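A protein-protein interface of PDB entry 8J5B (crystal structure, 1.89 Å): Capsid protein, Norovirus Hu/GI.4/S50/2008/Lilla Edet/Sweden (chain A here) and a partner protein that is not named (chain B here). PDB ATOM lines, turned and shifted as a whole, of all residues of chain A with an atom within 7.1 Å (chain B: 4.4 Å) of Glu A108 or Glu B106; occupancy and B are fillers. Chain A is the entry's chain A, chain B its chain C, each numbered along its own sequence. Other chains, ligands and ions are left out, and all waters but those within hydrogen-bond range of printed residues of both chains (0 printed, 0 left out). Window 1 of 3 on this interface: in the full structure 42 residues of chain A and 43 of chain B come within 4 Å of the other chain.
The side-chain carboxylate (OE1) of Glu B106 is in hydrogen-bond range of the side-chain amide nitrogen (NE2) of Gln A158, at 2.7 Å. NE2 of Gln A158 sits close to NE2 of Gln B156, 3.2 Å away. The side-chain carboxylate of Glu B106 sits close to the side-chain carboxylate of Glu A108, 2.4 Å away. The side-chain carboxylate (OE1) of Glu A108 lies close to the side-chain amide nitrogen (NE2) of Gln B156 (2.3 Å).
Of the 9 printed residues of chain B, 3 touch a printed residue of chain A. Hydrophobic or aromatic side chains of chain B that line the printed part of chain A: Ile B120. Printed residues of chain A that touch a printed residue of chain B: Glu A108, Ile A122, Gln A158 and Trp A159. Hydrophobic or aromatic side chains of chain A within 4 Å of the printed part of chain B: Ile A122 and Trp A159. Along chain A the printed residues that touch a printed residue of chain B span positions 108 to 159.
Among the printed residues, merely in contact across the chains: Ile A122 with Gln B156, Gln A158 with Ile B120 and Trp A159 with Ile B120.
Glu A108 touches two residues of chain B. Printed residues of chain B within 4 Å of Ile A122: Gln B156 (3.6 Å). Asn A125 touches none of the printed residues of chain B. Of the printed residues of chain B, Gln A158 touches Glu B106, Ile B120 and Gln B156. Printed residues of chain B within 4 Å of Trp A159: Ile B120. Glu B106 touches just these residues of chain A: Glu A108 (2.4 Å) and Gln A158 (2.7 Å). Met B107 touches none of the printed residues of chain A. The nearest printed residue of chain B that does not touch Glu A108 is Thr B154 (5.9 Å).
The backbone carbonyl oxygen of His A106 sits at hydrogen-bond distance from the backbone NH of Gln A158 (2.9 Å). The backbone NH (N) of His A106 is in hydrogen-bond range of the backbone carbonyl oxygen (O) of Trp A159 (2.8 Å). The backbone carbonyl oxygen of Glu A108 lies within hydrogen-bond range of the backbone NH of Thr A156 (3.0 Å). The side-chain carboxylate (OE1) of Glu A108 is in hydrogen-bond range of the side-chain amide nitrogen (NE2) of Gln A158 (3.5 Å). The backbone NH (N) of Thr B154 is in hydrogen-bond range of the backbone carbonyl oxygen (O) of Glu B106 (3.0 Å).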
ATOM      1  N   PHE A  65       4.279  -3.467 -24.615  1.00  0.00           N
ATOM      2  CA  PHE A  65       3.087  -4.332 -24.769  1.00  0.00           C
ATOM      3  C   PHE A  65       2.753  -4.942 -23.419  1.00  0.00           C
ATOM      4  O   PHE A  65       3.615  -5.069 -22.545  1.00  0.00           O
ATOM      5  CB  PHE A  65       3.335  -5.469 -25.781  1.00  0.00           C
ATOM      6  CG  PHE A  65       4.567  -6.296 -25.505  1.00  0.00           C
ATOM      7  CD1 PHE A  65       4.507  -7.427 -24.703  1.00  0.00           C
ATOM      8  CD2 PHE A  65       5.808  -5.911 -25.995  1.00  0.00           C
ATOM      9  CE1 PHE A  65       5.657  -8.159 -24.423  1.00  0.00           C
ATOM     10  CE2 PHE A  65       6.948  -6.646 -25.724  1.00  0.00           C
ATOM     11  CZ  PHE A  65       6.873  -7.765 -24.926  1.00  0.00           C
ATOM     12  N   HIS A 106      13.540  -9.196 -30.077  1.00  0.00           N
ATOM     13  CA  HIS A 106      13.996  -9.973 -28.908  1.00  0.00           C
ATOM     14  C   HIS A 106      13.520  -9.186 -27.701  1.00  0.00           C
ATOM     15  O   HIS A 106      14.000  -8.037 -27.492  1.00  0.00           O
ATOM     16  CB  HIS A 106      15.492 -10.254 -29.019  1.00  0.00           C
ATOM     17  CG  HIS A 106      15.847 -10.862 -30.341  1.00  0.00           C
ATOM     18  ND1 HIS A 106      15.969 -12.220 -30.521  1.00  0.00           N
ATOM     19  CD2 HIS A 106      16.066 -10.307 -31.557  1.00  0.00           C
ATOM     20  CE1 HIS A 106      16.284 -12.482 -31.777  1.00  0.00           C
ATOM     21  NE2 HIS A 106      16.342 -11.327 -32.439  1.00  0.00           N
ATOM     22  N   ILE A 107      12.523  -9.733 -27.017  1.00  0.00           N
ATOM     23  CA  ILE A 107      11.756  -8.973 -25.991  1.00  0.00           C
ATOM     24  C   ILE A 107      12.206  -9.400 -24.593  1.00  0.00           C
ATOM     25  O   ILE A 107      12.868 -10.469 -24.438  1.00  0.00           O
ATOM     26  CB  ILE A 107      10.234  -9.132 -26.154  1.00  0.00           C
ATOM     27  CG1 ILE A 107       9.774 -10.557 -25.835  1.00  0.00           C
ATOM     28  CG2 ILE A 107       9.758  -8.680 -27.523  1.00  0.00           C
ATOM     29  CD1 ILE A 107       8.324 -10.787 -26.127  1.00  0.00           C
ATOM     30  N   GLU A 108      11.864  -8.552 -23.625  1.00  0.00           N
ATOM     31  CA  GLU A 108      11.926  -8.859 -22.185  1.00  0.00           C
ATOM     32  C   GLU A 108      10.593  -8.414 -21.578  1.00  0.00           C
ATOM     33  O   GLU A 108       9.979  -7.435 -22.049  1.00  0.00           O
ATOM     34  CB  GLU A 108      13.146  -8.205 -21.548  1.00  0.00           C
ATOM     35  CG  GLU A 108      12.960  -6.737 -21.225  1.00  0.00           C
ATOM     36  CD  GLU A 108      14.129  -6.195 -20.436  1.00  0.00           C
ATOM     37  OE1 GLU A 108      14.558  -6.860 -19.462  1.00  0.00           O
ATOM     38  OE2 GLU A 108      14.630  -5.138 -20.817  1.00  0.00           O
ATOM     39  N   MET A 109      10.131  -9.174 -20.602  1.00  0.00           N
ATOM     40  CA  MET A 109       8.805  -8.976 -20.007  1.00  0.00           C
ATOM     41  C   MET A 109       8.800  -9.644 -18.637  1.00  0.00           C
ATOM     42  O   MET A 109       9.705 -10.466 -18.354  1.00  0.00           O
ATOM     43  CB  MET A 109       7.733  -9.578 -20.912  1.00  0.00           C
ATOM     44  CG  MET A 109       7.723 -11.093 -20.911  1.00  0.00           C
ATOM     45  SD  MET A 109       6.608 -11.757 -22.132  1.00  0.00           S
ATOM     46  CE  MET A 109       5.334 -10.509 -22.241  1.00  0.00           C
ATOM     47  N   SER A 110       7.846  -9.255 -17.808  1.00  0.00           N
ATOM     48  CA  SER A 110       7.737  -9.696 -16.401  1.00  0.00           C
ATOM     49  C   SER A 110       6.274  -9.615 -15.991  1.00  0.00           C
ATOM     50  O   SER A 110       5.525  -8.837 -16.615  1.00  0.00           O
ATOM     51  CB  SER A 110       8.648  -8.896 -15.499  1.00  0.00           C
ATOM     52  OG  SER A 110       8.175  -7.571 -15.335  1.00  0.00           O
ATOM     53  N   ILE A 122      12.443 -11.566 -14.902  1.00  0.00           N
ATOM     54  CA  ILE A 122      12.496 -11.222 -16.350  1.00  0.00           C
ATOM     55  C   ILE A 122      12.425 -12.526 -17.143  1.00  0.00           C
ATOM     56  O   ILE A 122      13.237 -13.432 -16.896  1.00  0.00           O
ATOM     57  CB  ILE A 122      13.724 -10.375 -16.729  1.00  0.00           C
ATOM     58  CG1 ILE A 122      13.896  -9.152 -15.827  1.00  0.00           C
ATOM     59  CG2 ILE A 122      13.642  -9.948 -18.189  1.00  0.00           C
ATOM     60  CD1 ILE A 122      12.817  -8.130 -15.986  1.00  0.00           C
ATOM     61  N   VAL A 123      11.453 -12.610 -18.043  1.00  0.00           N
ATOM     62  CA  VAL A 123      11.388 -13.652 -19.102  1.00  0.00           C
ATOM     63  C   VAL A 123      11.806 -12.973 -20.414  1.00  0.00           C
ATOM     64  O   VAL A 123      11.317 -11.855 -20.679  1.00  0.00           O
ATOM     65  CB  VAL A 123       9.995 -14.312 -19.162  1.00  0.00           C
ATOM     66  CG1 VAL A 123       9.969 -15.462 -20.165  1.00  0.00           C
ATOM     67  CG2 VAL A 123       9.546 -14.820 -17.793  1.00  0.00           C
ATOM     68  N   THR A 124      12.759 -13.578 -21.142  1.00  0.00           N
ATOM     69  CA  THR A 124      13.143 -13.181 -22.526  1.00  0.00           C
ATOM     70  C   THR A 124      12.468 -14.140 -23.514  1.00  0.00           C
ATOM     71  O   THR A 124      12.012 -15.255 -23.111  1.00  0.00           O
ATOM     72  CB  THR A 124      14.662 -13.067 -22.712  1.00  0.00           C
ATOM     73  OG1 THR A 124      15.299 -14.331 -22.550  1.00  0.00           O
ATOM     74  CG2 THR A 124      15.296 -12.078 -21.755  1.00  0.00           C
ATOM     75  N   ASN A 125      12.334 -13.679 -24.753  1.00  0.00           N
ATOM     76  CA  ASN A 125      11.576 -14.376 -25.816  1.00  0.00           C
ATOM     77  C   ASN A 125      11.736 -13.561 -27.104  1.00  0.00           C
ATOM     78  O   ASN A 125      12.425 -12.514 -27.074  1.00  0.00           O
ATOM     79  CB  ASN A 125      10.126 -14.597 -25.400  1.00  0.00           C
ATOM     80  CG  ASN A 125       9.572 -15.930 -25.867  1.00  0.00           C
ATOM     81  OD1 ASN A 125       9.665 -16.261 -27.046  1.00  0.00           O
ATOM     82  ND2 ASN A 125       8.966 -16.693 -24.962  1.00  0.00           N
ATOM     83  N   TYR A 153       1.560 -10.169 -18.307  1.00  0.00           N
ATOM     84  CA  TYR A 153       2.959  -9.781 -18.616  1.00  0.00           C
ATOM     85  C   TYR A 153       2.980  -8.404 -19.290  1.00  0.00           C
ATOM     86  O   TYR A 153       2.110  -8.058 -20.079  1.00  0.00           O
ATOM     87  CB  TYR A 153       3.664 -10.816 -19.502  1.00  0.00           C
ATOM     88  CG  TYR A 153       4.207 -12.053 -18.825  1.00  0.00           C
ATOM     89  CD1 TYR A 153       3.414 -13.171 -18.633  1.00  0.00           C
ATOM     90  CD2 TYR A 153       5.514 -12.111 -18.387  1.00  0.00           C
ATOM     91  CE1 TYR A 153       3.899 -14.304 -18.004  1.00  0.00           C
ATOM     92  CE2 TYR A 153       6.031 -13.247 -17.785  1.00  0.00           C
ATOM     93  CZ  TYR A 153       5.221 -14.354 -17.595  1.00  0.00           C
ATOM     94  OH  TYR A 153       5.717 -15.482 -17.005  1.00  0.00           O
ATOM     95  N   ILE A 154       3.990  -7.626 -18.952  1.00  0.00           N
ATOM     96  CA  ILE A 154       4.248  -6.288 -19.556  1.00  0.00           C
ATOM     97  C   ILE A 154       5.689  -6.358 -20.015  1.00  0.00           C
ATOM     98  O   ILE A 154       6.529  -6.915 -19.246  1.00  0.00           O
ATOM     99  CB  ILE A 154       4.011  -5.111 -18.577  1.00  0.00           C
ATOM    100  CG1 ILE A 154       4.229  -3.758 -19.262  1.00  0.00           C
ATOM    101  CG2 ILE A 154       4.888  -5.203 -17.335  1.00  0.00           C
ATOM    102  CD1 ILE A 154       3.642  -2.600 -18.486  1.00  0.00           C
ATOM    103  N   GLY A 155       5.977  -5.852 -21.205  1.00  0.00           N
ATOM    104  CA  GLY A 155       7.367  -5.906 -21.678  1.00  0.00           C
ATOM    105  C   GLY A 155       7.643  -4.912 -22.781  1.00  0.00           C
ATOM    106  O   GLY A 155       6.750  -4.107 -23.127  1.00  0.00           O
ATOM    107  N   THR A 156       8.854  -5.015 -23.313  1.00  0.00           N
ATOM    108  CA  THR A 156       9.384  -4.133 -24.377  1.00  0.00           C
ATOM    109  C   THR A 156      10.247  -4.944 -25.348  1.00  0.00           C
ATOM    110  O   THR A 156      10.466  -6.171 -25.120  1.00  0.00           O
ATOM    111  CB  THR A 156      10.158  -2.970 -23.744  1.00  0.00           C
ATOM    112  OG1 THR A 156      10.553  -2.083 -24.804  1.00  0.00           O
ATOM    113  CG2 THR A 156      11.345  -3.428 -22.922  1.00  0.00           C
ATOM    114  N   ILE A 157      10.750  -4.262 -26.377  1.00  0.00           N
ATOM    115  CA  ILE A 157      11.804  -4.775 -27.282  1.00  0.00           C
ATOM    116  C   ILE A 157      13.150  -4.446 -26.640  1.00  0.00           C
ATOM    117  O   ILE A 157      13.471  -3.266 -26.491  1.00  0.00           O
ATOM    118  CB  ILE A 157      11.632  -4.185 -28.694  1.00  0.00           C
ATOM    119  CG1 ILE A 157      10.234  -4.498 -29.239  1.00  0.00           C
ATOM    120  CG2 ILE A 157      12.745  -4.706 -29.593  1.00  0.00           C
ATOM    121  CD1 ILE A 157       9.937  -3.965 -30.618  1.00  0.00           C
ATOM    122  N   GLN A 158      13.869  -5.477 -26.221  1.00  0.00           N
ATOM    123  CA  GLN A 158      15.212  -5.374 -25.635  1.00  0.00           C
ATOM    124  C   GLN A 158      16.235  -5.115 -26.752  1.00  0.00           C
ATOM    125  O   GLN A 158      17.134  -4.277 -26.549  1.00  0.00           O
ATOM    126  CB  GLN A 158      15.443  -6.657 -24.867  1.00  0.00           C
ATOM    127  CG  GLN A 158      16.554  -6.534 -23.860  1.00  0.00           C
ATOM    128  CD  GLN A 158      16.742  -7.862 -23.187  1.00  0.00           C
ATOM    129  OE1 GLN A 158      16.776  -8.907 -23.848  1.00  0.00           O
ATOM    130  NE2 GLN A 158      16.867  -7.828 -21.871  1.00  0.00           N
ATOM    131  N   TRP A 159      16.107  -5.829 -27.880  1.00  0.00           N
ATOM    132  CA  TRP A 159      17.016  -5.722 -29.053  1.00  0.00           C
ATOM    133  C   TRP A 159      16.345  -6.270 -30.322  1.00  0.00           C
ATOM    134  O   TRP A 159      15.396  -7.065 -30.216  1.00  0.00           O
ATOM    135  CB  TRP A 159      18.378  -6.375 -28.778  1.00  0.00           C
ATOM    136  CG  TRP A 159      18.367  -7.843 -28.473  1.00  0.00           C
ATOM    137  CD1 TRP A 159      17.956  -8.443 -27.314  1.00  0.00           C
ATOM    138  CD2 TRP A 159      18.838  -8.905 -29.324  1.00  0.00           C
ATOM    139  NE1 TRP A 159      18.122  -9.799 -27.390  1.00  0.00           N
ATOM    140  CE2 TRP A 159      18.660 -10.118 -28.611  1.00  0.00           C
ATOM    141  CE3 TRP A 159      19.361  -8.963 -30.623  1.00  0.00           C
ATOM    142  CZ2 TRP A 159      19.003 -11.361 -29.159  1.00  0.00           C
ATOM    143  CZ3 TRP A 159      19.701 -10.185 -31.164  1.00  0.00           C
ATOM    144  CH2 TRP A 159      19.525 -11.370 -30.435  1.00  0.00           C
ATOM    145  N   PHE B  63      22.307   4.914 -17.271  1.00  0.00           N
ATOM    146  CA  PHE B  63      23.747   5.147 -17.015  1.00  0.00           C
ATOM    147  C   PHE B  63      24.506   4.853 -18.312  1.00  0.00           C
ATOM    148  O   PHE B  63      23.985   4.125 -19.210  1.00  0.00           O
ATOM    149  CB  PHE B  63      24.189   4.290 -15.824  1.00  0.00           C
ATOM    150  CG  PHE B  63      23.993   2.809 -16.011  1.00  0.00           C
ATOM    151  CD1 PHE B  63      24.852   2.071 -16.801  1.00  0.00           C
ATOM    152  CD2 PHE B  63      22.951   2.150 -15.382  1.00  0.00           C
ATOM    153  CE1 PHE B  63      24.658   0.707 -16.975  1.00  0.00           C
ATOM    154  CE2 PHE B  63      22.761   0.788 -15.552  1.00  0.00           C
ATOM    155  CZ  PHE B  63      23.621   0.064 -16.337  1.00  0.00           C
ATOM    156  N   ILE B 105      20.953  -4.833 -13.663  1.00  0.00           N
ATOM    157  CA  ILE B 105      21.039  -3.891 -14.813  1.00  0.00           C
ATOM    158  C   ILE B 105      21.085  -4.673 -16.138  1.00  0.00           C
ATOM    159  O   ILE B 105      21.474  -5.870 -16.166  1.00  0.00           O
ATOM    160  CB  ILE B 105      22.251  -2.961 -14.644  1.00  0.00           C
ATOM    161  CG1 ILE B 105      23.555  -3.756 -14.557  1.00  0.00           C
ATOM    162  CG2 ILE B 105      22.080  -2.056 -13.438  1.00  0.00           C
ATOM    163  CD1 ILE B 105      24.819  -2.927 -14.596  1.00  0.00           C
ATOM    164  N   GLU B 106      20.679  -4.025 -17.216  1.00  0.00           N
ATOM    165  CA  GLU B 106      20.948  -4.522 -18.576  1.00  0.00           C
ATOM    166  C   GLU B 106      21.586  -3.357 -19.342  1.00  0.00           C
ATOM    167  O   GLU B 106      21.377  -2.206 -18.966  1.00  0.00           O
ATOM    168  CB  GLU B 106      19.671  -5.101 -19.163  1.00  0.00           C
ATOM    169  CG  GLU B 106      18.568  -4.087 -19.307  1.00  0.00           C
ATOM    170  CD  GLU B 106      17.557  -4.418 -20.386  1.00  0.00           C
ATOM    171  OE1 GLU B 106      17.799  -5.354 -21.174  1.00  0.00           O
ATOM    172  OE2 GLU B 106      16.538  -3.735 -20.432  1.00  0.00           O
ATOM    173  N   MET B 107      22.429  -3.671 -20.310  1.00  0.00           N
ATOM    174  CA  MET B 107      23.229  -2.663 -21.024  1.00  0.00           C
ATOM    175  C   MET B 107      23.817  -3.300 -22.282  1.00  0.00           C
ATOM    176  O   MET B 107      23.807  -4.534 -22.428  1.00  0.00           O
ATOM    177  CB  MET B 107      24.344  -2.130 -20.125  1.00  0.00           C
ATOM    178  CG  MET B 107      25.382  -3.147 -19.743  1.00  0.00           C
ATOM    179  SD  MET B 107      26.552  -2.374 -18.638  1.00  0.00           S
ATOM    180  CE  MET B 107      27.701  -3.716 -18.347  1.00  0.00           C
ATOM    181  N   ILE B 120      23.061  -7.670 -25.566  1.00  0.00           N
ATOM    182  CA  ILE B 120      22.658  -7.324 -24.178  1.00  0.00           C
ATOM    183  C   ILE B 120      23.575  -8.032 -23.197  1.00  0.00           C
ATOM    184  O   ILE B 120      23.698  -9.230 -23.279  1.00  0.00           O
ATOM    185  CB  ILE B 120      21.188  -7.660 -23.893  1.00  0.00           C
ATOM    186  CG1 ILE B 120      20.263  -6.940 -24.872  1.00  0.00           C
ATOM    187  CG2 ILE B 120      20.845  -7.327 -22.448  1.00  0.00           C
ATOM    188  CD1 ILE B 120      20.589  -5.487 -25.071  1.00  0.00           C
ATOM    189  N   VAL B 121      24.156  -7.275 -22.275  1.00  0.00           N
ATOM    190  CA  VAL B 121      24.864  -7.825 -21.092  1.00  0.00           C
ATOM    191  C   VAL B 121      23.994  -7.505 -19.874  1.00  0.00           C
ATOM    192  O   VAL B 121      23.706  -6.320 -19.667  1.00  0.00           O
ATOM    193  CB  VAL B 121      26.276  -7.224 -20.974  1.00  0.00           C
ATOM    194  CG1 VAL B 121      26.970  -7.650 -19.682  1.00  0.00           C
ATOM    195  CG2 VAL B 121      27.136  -7.566 -22.186  1.00  0.00           C
ATOM    196  N   GLY B 153      22.876   1.680 -20.416  1.00  0.00           N
ATOM    197  CA  GLY B 153      21.978   0.687 -19.796  1.00  0.00           C
ATOM    198  C   GLY B 153      20.996   1.311 -18.824  1.00  0.00           C
ATOM    199  O   GLY B 153      20.901   2.543 -18.731  1.00  0.00           O
ATOM    200  N   THR B 154      20.312   0.444 -18.082  1.00  0.00           N
ATOM    201  CA  THR B 154      19.150   0.798 -17.252  1.00  0.00           C
ATOM    202  C   THR B 154      18.984  -0.287 -16.190  1.00  0.00           C
ATOM    203  O   THR B 154      19.612  -1.360 -16.334  1.00  0.00           O
ATOM    204  CB  THR B 154      17.900   0.975 -18.133  1.00  0.00           C
ATOM    205  OG1 THR B 154      16.937   1.556 -17.257  1.00  0.00           O
ATOM    206  CG2 THR B 154      17.364  -0.307 -18.740  1.00  0.00           C
ATOM    207  N   GLN B 156      17.077  -3.199 -14.870  1.00  0.00           N
ATOM    208  CA  GLN B 156      16.121  -4.175 -15.423  1.00  0.00           C
ATOM    209  C   GLN B 156      15.182  -4.651 -14.312  1.00  0.00           C
ATOM    210  O   GLN B 156      13.971  -4.739 -14.563  1.00  0.00           O
ATOM    211  CB  GLN B 156      16.892  -5.345 -16.034  1.00  0.00           C
ATOM    212  CG  GLN B 156      15.994  -6.349 -16.734  1.00  0.00           C
ATOM    213  CD  GLN B 156      16.825  -7.422 -17.386  1.00  0.00           C
ATOM    214  OE1 GLN B 156      17.707  -7.994 -16.754  1.00  0.00           O
ATOM    215  NE2 GLN B 156      16.584  -7.657 -18.669  1.00  0.00           N
